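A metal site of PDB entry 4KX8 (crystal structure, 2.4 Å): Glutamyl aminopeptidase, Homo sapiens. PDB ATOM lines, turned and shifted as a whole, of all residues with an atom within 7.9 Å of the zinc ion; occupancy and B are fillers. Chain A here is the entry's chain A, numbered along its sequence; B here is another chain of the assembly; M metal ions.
O1 of L2O 1 of chain B sits close to the side-chain carboxylate of Glu 319.
OE1 of Glu 285 sits at hydrogen-bond distance from N of L2O 1 of chain B (3.0 Å).
OE1 of Glu 148 sits at hydrogen-bond distance from N of L2O 1 of chain B, at 2.5 Å.
N of L2O 1 of chain B sits at hydrogen-bond distance from the side-chain sulfur of Met 284 (3.7 Å).
The side-chain hydroxyl of Tyr 404 lies close to the side-chain carboxylate of Glu 341, 3.2 Å away.
OG of Ser 345 lies within hydrogen-bond range of O of Glu 341 (3.1 Å).
ND1 of His 318 is in hydrogen-bond range of OE2 of Glu 348, at 2.8 Å.
O of Phe 325 is in hydrogen-bond range of ND1 of His 322.
OE1 of Glu 319 touches the zinc ion (3.9 Å).
Tyr 404 touches the zinc ion.
The nearest printed residue that does not touch the zinc ion is Ala 344 (4.3 Å).
The zinc ion is bound by O1 of L2O 1 of chain B.
OE1 of Glu 341 binds the zinc ion (2.1 Å).
NE2 of His 318 binds the zinc ion, 2.2 Å away.
The zinc ion is bound by NE2 of His 322 (2.3 Å).
The zinc ion has four donor atoms within binding distance.
Slightly farther from the zinc ion lies O of L2O 1 of chain B (2.8 Å).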
ATOM      1  N   GLU A 148      12.044   5.889 -15.700  1.00  0.00           N
ATOM      2  CA  GLU A 148      13.246   6.740 -15.706  1.00  0.00           C
ATOM      3  C   GLU A 148      12.951   8.181 -16.132  1.00  0.00           C
ATOM      4  O   GLU A 148      12.314   8.406 -17.156  1.00  0.00           O
ATOM      5  CB  GLU A 148      14.334   6.139 -16.596  1.00  0.00           C
ATOM      6  CG  GLU A 148      15.726   6.660 -16.291  1.00  0.00           C
ATOM      7  CD  GLU A 148      16.790   5.815 -16.944  1.00  0.00           C
ATOM      8  OE1 GLU A 148      16.488   5.146 -17.962  1.00  0.00           O
ATOM      9  OE2 GLU A 148      17.944   5.832 -16.445  1.00  0.00           O
ATOM     10  N   ALA A 283      13.041   3.821 -26.045  1.00  0.00           N
ATOM     11  CA  ALA A 283      13.212   2.508 -25.452  1.00  0.00           C
ATOM     12  C   ALA A 283      13.743   2.634 -24.019  1.00  0.00           C
ATOM     13  O   ALA A 283      14.393   3.639 -23.690  1.00  0.00           O
ATOM     14  CB  ALA A 283      14.156   1.660 -26.285  1.00  0.00           C
ATOM     15  N   MET A 284      13.477   1.615 -23.196  1.00  0.00           N
ATOM     16  CA  MET A 284      13.834   1.634 -21.775  1.00  0.00           C
ATOM     17  C   MET A 284      14.371   0.267 -21.331  1.00  0.00           C
ATOM     18  O   MET A 284      13.775  -0.768 -21.625  1.00  0.00           O
ATOM     19  CB  MET A 284      12.610   2.054 -20.951  1.00  0.00           C
ATOM     20  CG  MET A 284      12.849   2.223 -19.481  1.00  0.00           C
ATOM     21  SD  MET A 284      14.372   3.109 -19.157  1.00  0.00           S
ATOM     22  CE  MET A 284      14.642   2.609 -17.464  1.00  0.00           C
ATOM     23  N   GLU A 285      15.484   0.269 -20.615  1.00  0.00           N
ATOM     24  CA  GLU A 285      16.276  -0.942 -20.370  1.00  0.00           C
ATOM     25  C   GLU A 285      15.824  -1.788 -19.173  1.00  0.00           C
ATOM     26  O   GLU A 285      16.613  -2.586 -18.648  1.00  0.00           O
ATOM     27  CB  GLU A 285      17.762  -0.596 -20.201  1.00  0.00           C
ATOM     28  CG  GLU A 285      18.097   0.212 -18.952  1.00  0.00           C
ATOM     29  CD  GLU A 285      18.095   1.717 -19.206  1.00  0.00           C
ATOM     30  OE1 GLU A 285      17.316   2.184 -20.049  1.00  0.00           O
ATOM     31  OE2 GLU A 285      18.874   2.435 -18.533  1.00  0.00           O
ATOM     32  N   VAL A 315      19.498   0.395 -31.360  1.00  0.00           N
ATOM     33  CA  VAL A 315      18.730   0.623 -30.145  1.00  0.00           C
ATOM     34  C   VAL A 315      18.674  -0.660 -29.321  1.00  0.00           C
ATOM     35  O   VAL A 315      18.822  -0.625 -28.102  1.00  0.00           O
ATOM     36  CB  VAL A 315      17.325   1.177 -30.417  1.00  0.00           C
ATOM     37  CG1 VAL A 315      16.547   1.333 -29.130  1.00  0.00           C
ATOM     38  CG2 VAL A 315      17.418   2.519 -31.139  1.00  0.00           C
ATOM     39  N   HIS A 318      22.060  -0.918 -27.837  1.00  0.00           N
ATOM     40  CA  HIS A 318      22.117   0.105 -26.786  1.00  0.00           C
ATOM     41  C   HIS A 318      21.484  -0.410 -25.513  1.00  0.00           C
ATOM     42  O   HIS A 318      22.077  -0.380 -24.436  1.00  0.00           O
ATOM     43  CB  HIS A 318      21.384   1.374 -27.263  1.00  0.00           C
ATOM     44  CG  HIS A 318      21.435   2.517 -26.294  1.00  0.00           C
ATOM     45  ND1 HIS A 318      22.262   3.602 -26.477  1.00  0.00           N
ATOM     46  CD2 HIS A 318      20.757   2.749 -25.144  1.00  0.00           C
ATOM     47  CE1 HIS A 318      22.111   4.451 -25.481  1.00  0.00           C
ATOM     48  NE2 HIS A 318      21.196   3.962 -24.656  1.00  0.00           N
ATOM     49  N   GLU A 319      20.241  -0.888 -25.648  1.00  0.00           N
ATOM     50  CA  GLU A 319      19.458  -1.360 -24.516  1.00  0.00           C
ATOM     51  C   GLU A 319      20.084  -2.603 -23.894  1.00  0.00           C
ATOM     52  O   GLU A 319      19.936  -2.823 -22.691  1.00  0.00           O
ATOM     53  CB  GLU A 319      18.013  -1.614 -24.955  1.00  0.00           C
ATOM     54  CG  GLU A 319      16.986  -0.552 -24.561  1.00  0.00           C
ATOM     55  CD  GLU A 319      17.545   0.858 -24.417  1.00  0.00           C
ATOM     56  OE1 GLU A 319      17.872   1.258 -23.279  1.00  0.00           O
ATOM     57  OE2 GLU A 319      17.650   1.575 -25.424  1.00  0.00           O
ATOM     58  N   VAL A 321      23.404  -3.127 -23.749  1.00  0.00           N
ATOM     59  CA  VAL A 321      24.572  -2.661 -22.987  1.00  0.00           C
ATOM     60  C   VAL A 321      24.182  -2.345 -21.550  1.00  0.00           C
ATOM     61  O   VAL A 321      24.922  -2.625 -20.608  1.00  0.00           O
ATOM     62  CB  VAL A 321      25.243  -1.424 -23.615  1.00  0.00           C
ATOM     63  CG1 VAL A 321      26.442  -1.006 -22.778  1.00  0.00           C
ATOM     64  CG2 VAL A 321      25.691  -1.721 -25.041  1.00  0.00           C
ATOM     65  N   HIS A 322      22.994  -1.767 -21.400  1.00  0.00           N
ATOM     66  CA  HIS A 322      22.506  -1.367 -20.090  1.00  0.00           C
ATOM     67  C   HIS A 322      22.317  -2.519 -19.103  1.00  0.00           C
ATOM     68  O   HIS A 322      22.334  -2.306 -17.884  1.00  0.00           O
ATOM     69  CB  HIS A 322      21.214  -0.577 -20.218  1.00  0.00           C
ATOM     70  CG  HIS A 322      21.423   0.870 -20.567  1.00  0.00           C
ATOM     71  ND1 HIS A 322      22.227   1.711 -19.820  1.00  0.00           N
ATOM     72  CD2 HIS A 322      20.915   1.625 -21.562  1.00  0.00           C
ATOM     73  CE1 HIS A 322      22.215   2.911 -20.362  1.00  0.00           C
ATOM     74  NE2 HIS A 322      21.421   2.895 -21.418  1.00  0.00           N
ATOM     75  N   PHE A 325      25.963  -2.231 -18.117  1.00  0.00           N
ATOM     76  CA  PHE A 325      26.235  -0.855 -17.707  1.00  0.00           C
ATOM     77  C   PHE A 325      24.977  -0.054 -17.491  1.00  0.00           C
ATOM     78  O   PHE A 325      24.356   0.421 -18.443  1.00  0.00           O
ATOM     79  CB  PHE A 325      27.154  -0.168 -18.708  1.00  0.00           C
ATOM     80  CG  PHE A 325      28.572  -0.563 -18.557  1.00  0.00           C
ATOM     81  CD1 PHE A 325      29.396   0.063 -17.625  1.00  0.00           C
ATOM     82  CD2 PHE A 325      29.107  -1.586 -19.336  1.00  0.00           C
ATOM     83  CE1 PHE A 325      30.718  -0.307 -17.474  1.00  0.00           C
ATOM     84  CE2 PHE A 325      30.427  -1.966 -19.188  1.00  0.00           C
ATOM     85  CZ  PHE A 325      31.235  -1.326 -18.261  1.00  0.00           C
ATOM     86  N   LEU A 337      25.153  10.259 -14.721  1.00  0.00           N
ATOM     87  CA  LEU A 337      24.320   9.579 -15.716  1.00  0.00           C
ATOM     88  C   LEU A 337      25.085   9.082 -16.943  1.00  0.00           C
ATOM     89  O   LEU A 337      24.679   8.105 -17.573  1.00  0.00           O
ATOM     90  CB  LEU A 337      23.179  10.495 -16.175  1.00  0.00           C
ATOM     91  CG  LEU A 337      22.248   9.985 -17.269  1.00  0.00           C
ATOM     92  CD1 LEU A 337      21.484   8.746 -16.806  1.00  0.00           C
ATOM     93  CD2 LEU A 337      21.296  11.080 -17.681  1.00  0.00           C
ATOM     94  N   ASN A 340      25.983   5.435 -17.390  1.00  0.00           N
ATOM     95  CA  ASN A 340      24.982   4.595 -18.035  1.00  0.00           C
ATOM     96  C   ASN A 340      24.925   4.866 -19.522  1.00  0.00           C
ATOM     97  O   ASN A 340      25.243   4.000 -20.328  1.00  0.00           O
ATOM     98  CB  ASN A 340      23.580   4.814 -17.440  1.00  0.00           C
ATOM     99  CG  ASN A 340      23.455   4.326 -16.015  1.00  0.00           C
ATOM    100  OD1 ASN A 340      22.356   4.213 -15.488  1.00  0.00           O
ATOM    101  ND2 ASN A 340      24.580   4.044 -15.375  1.00  0.00           N
ATOM    102  N   GLU A 341      24.545   6.090 -19.878  1.00  0.00           N
ATOM    103  CA  GLU A 341      24.191   6.427 -21.257  1.00  0.00           C
ATOM    104  C   GLU A 341      25.374   6.565 -22.207  1.00  0.00           C
ATOM    105  O   GLU A 341      25.287   6.173 -23.387  1.00  0.00           O
ATOM    106  CB  GLU A 341      23.337   7.689 -21.317  1.00  0.00           C
ATOM    107  CG  GLU A 341      22.080   7.637 -20.446  1.00  0.00           C
ATOM    108  CD  GLU A 341      21.144   6.505 -20.805  1.00  0.00           C
ATOM    109  OE1 GLU A 341      21.263   5.908 -21.893  1.00  0.00           O
ATOM    110  OE2 GLU A 341      20.243   6.206 -19.990  1.00  0.00           O
ATOM    111  N   GLY A 342      26.461   7.140 -21.710  1.00  0.00           N
ATOM    112  CA  GLY A 342      27.680   7.269 -22.503  1.00  0.00           C
ATOM    113  C   GLY A 342      28.211   5.906 -22.905  1.00  0.00           C
ATOM    114  O   GLY A 342      28.584   5.688 -24.055  1.00  0.00           O
ATOM    115  N   PHE A 343      28.225   4.991 -21.933  1.00  0.00           N
ATOM    116  CA  PHE A 343      28.720   3.615 -22.125  1.00  0.00           C
ATOM    117  C   PHE A 343      27.844   2.823 -23.074  1.00  0.00           C
ATOM    118  O   PHE A 343      28.342   2.047 -23.890  1.00  0.00           O
ATOM    119  CB  PHE A 343      28.817   2.894 -20.779  1.00  0.00           C
ATOM    120  CG  PHE A 343      29.978   3.330 -19.947  1.00  0.00           C
ATOM    121  CD1 PHE A 343      30.072   4.631 -19.475  1.00  0.00           C
ATOM    122  CD2 PHE A 343      30.993   2.435 -19.643  1.00  0.00           C
ATOM    123  CE1 PHE A 343      31.150   5.034 -18.706  1.00  0.00           C
ATOM    124  CE2 PHE A 343      32.077   2.817 -18.875  1.00  0.00           C
ATOM    125  CZ  PHE A 343      32.150   4.121 -18.403  1.00  0.00           C
ATOM    126  N   ALA A 344      26.532   3.022 -22.966  1.00  0.00           N
ATOM    127  CA  ALA A 344      25.570   2.408 -23.867  1.00  0.00           C
ATOM    128  C   ALA A 344      25.750   2.929 -25.290  1.00  0.00           C
ATOM    129  O   ALA A 344      25.758   2.149 -26.233  1.00  0.00           O
ATOM    130  CB  ALA A 344      24.157   2.649 -23.378  1.00  0.00           C
ATOM    131  N   SER A 345      25.917   4.254 -25.410  1.00  0.00           N
ATOM    132  CA  SER A 345      26.145   4.911 -26.709  1.00  0.00           C
ATOM    133  C   SER A 345      27.475   4.512 -27.334  1.00  0.00           C
ATOM    134  O   SER A 345      27.636   4.613 -28.566  1.00  0.00           O
ATOM    135  CB  SER A 345      26.053   6.448 -26.590  1.00  0.00           C
ATOM    136  OG  SER A 345      24.714   6.854 -26.349  1.00  0.00           O
ATOM    137  N   GLU A 348      27.098   0.214 -28.026  1.00  0.00           N
ATOM    138  CA  GLU A 348      26.088  -0.077 -29.036  1.00  0.00           C
ATOM    139  C   GLU A 348      26.755  -0.299 -30.397  1.00  0.00           C
ATOM    140  O   GLU A 348      26.362  -1.182 -31.139  1.00  0.00           O
ATOM    141  CB  GLU A 348      25.032   1.020 -29.112  1.00  0.00           C
ATOM    142  CG  GLU A 348      25.550   2.365 -29.593  1.00  0.00           C
ATOM    143  CD  GLU A 348      24.459   3.415 -29.743  1.00  0.00           C
ATOM    144  OE1 GLU A 348      24.593   4.251 -30.664  1.00  0.00           O
ATOM    145  OE2 GLU A 348      23.471   3.415 -28.971  1.00  0.00           O
ATOM    146  N   PHE A 399      19.422  13.869 -19.903  1.00  0.00           N
ATOM    147  CA  PHE A 399      19.397  12.814 -20.898  1.00  0.00           C
ATOM    148  C   PHE A 399      19.572  13.480 -22.270  1.00  0.00           C
ATOM    149  O   PHE A 399      18.622  13.639 -23.015  1.00  0.00           O
ATOM    150  CB  PHE A 399      18.084  12.027 -20.834  1.00  0.00           C
ATOM    151  CG  PHE A 399      17.963  11.158 -19.624  1.00  0.00           C
ATOM    152  CD1 PHE A 399      17.471  11.666 -18.433  1.00  0.00           C
ATOM    153  CD2 PHE A 399      18.376   9.825 -19.667  1.00  0.00           C
ATOM    154  CE1 PHE A 399      17.385  10.859 -17.307  1.00  0.00           C
ATOM    155  CE2 PHE A 399      18.301   9.030 -18.556  1.00  0.00           C
ATOM    156  CZ  PHE A 399      17.799   9.531 -17.372  1.00  0.00           C
ATOM    157  N   TYR A 404      25.131  11.332 -23.646  1.00  0.00           N
ATOM    158  CA  TYR A 404      25.219  10.270 -24.639  1.00  0.00           C
ATOM    159  C   TYR A 404      26.404  10.450 -25.591  1.00  0.00           C
ATOM    160  O   TYR A 404      27.344   9.657 -25.596  1.00  0.00           O
ATOM    161  CB  TYR A 404      23.936  10.234 -25.477  1.00  0.00           C
ATOM    162  CG  TYR A 404      22.711   9.679 -24.810  1.00  0.00           C
ATOM    163  CD1 TYR A 404      22.052  10.389 -23.793  1.00  0.00           C
ATOM    164  CD2 TYR A 404      22.165   8.470 -25.217  1.00  0.00           C
ATOM    165  CE1 TYR A 404      20.909   9.885 -23.197  1.00  0.00           C
ATOM    166  CE2 TYR A 404      21.023   7.965 -24.621  1.00  0.00           C
ATOM    167  CZ  TYR A 404      20.410   8.684 -23.624  1.00  0.00           C
ATOM    168  OH  TYR A 404      19.286   8.181 -23.041  1.00  0.00           O
ATOM    169  N   L2O B   1      17.253   5.164 -20.387  1.00  0.00           N
ATOM    170  CA  L2O B   1      16.799   5.724 -21.682  1.00  0.00           C
ATOM    171  C2  L2O B   1      15.290   6.107 -21.746  1.00  0.00           C
ATOM    172  C3  L2O B   1      15.007   7.399 -20.972  1.00  0.00           C
ATOM    173  C4  L2O B   1      15.097   8.613 -21.907  1.00  0.00           C
ATOM    174  C5  L2O B   1      13.586   7.333 -20.366  1.00  0.00           C
ATOM    175  C6  L2O B   1      17.086   4.778 -22.856  1.00  0.00           C
ATOM    176  O1  L2O B   1      18.280   4.001 -22.685  1.00  0.00           O
ATOM    177  C   L2O B   1      17.415   5.645 -24.023  1.00  0.00           C
ATOM    178  O   L2O B   1      18.523   6.227 -23.997  1.00  0.00           O
ATOM    179  N   VAL B   2      16.739   5.187 -25.210  1.00  0.00           N
ATOM    180  CA  VAL B   2      16.936   6.100 -26.289  1.00  0.00           C
ATOM    181  C   VAL B   2      15.783   7.067 -26.190  1.00  0.00           C
ATOM    182  O   VAL B   2      14.679   6.690 -25.836  1.00  0.00           O
ATOM    183  CB  VAL B   2      16.984   5.350 -27.609  1.00  0.00           C
ATOM    184  CG1 VAL B   2      17.079   6.309 -28.756  1.00  0.00           C
ATOM    185  CG2 VAL B   2      18.210   4.468 -27.639  1.00  0.00           C
ATOM    186  N   VAL B   3      16.056   8.332 -26.449  1.00  0.00           N
ATOM    187  CA  VAL B   3      15.101   9.373 -26.240  1.00  0.00           C
ATOM    188  C   VAL B   3      14.056   9.441 -27.344  1.00  0.00           C
ATOM    189  O   VAL B   3      13.103  10.108 -27.223  1.00  0.00           O
ATOM    190  CB  VAL B   3      15.847  10.717 -26.147  1.00  0.00           C
ATOM    191  CG1 VAL B   3      14.900  11.895 -26.159  1.00  0.00           C
ATOM    192  CG2 VAL B   3      16.715  10.756 -24.920  1.00  0.00           C
HETATM  193 ZN    ZN M   1      20.256   4.341 -22.750  1.00  0.00          ZN
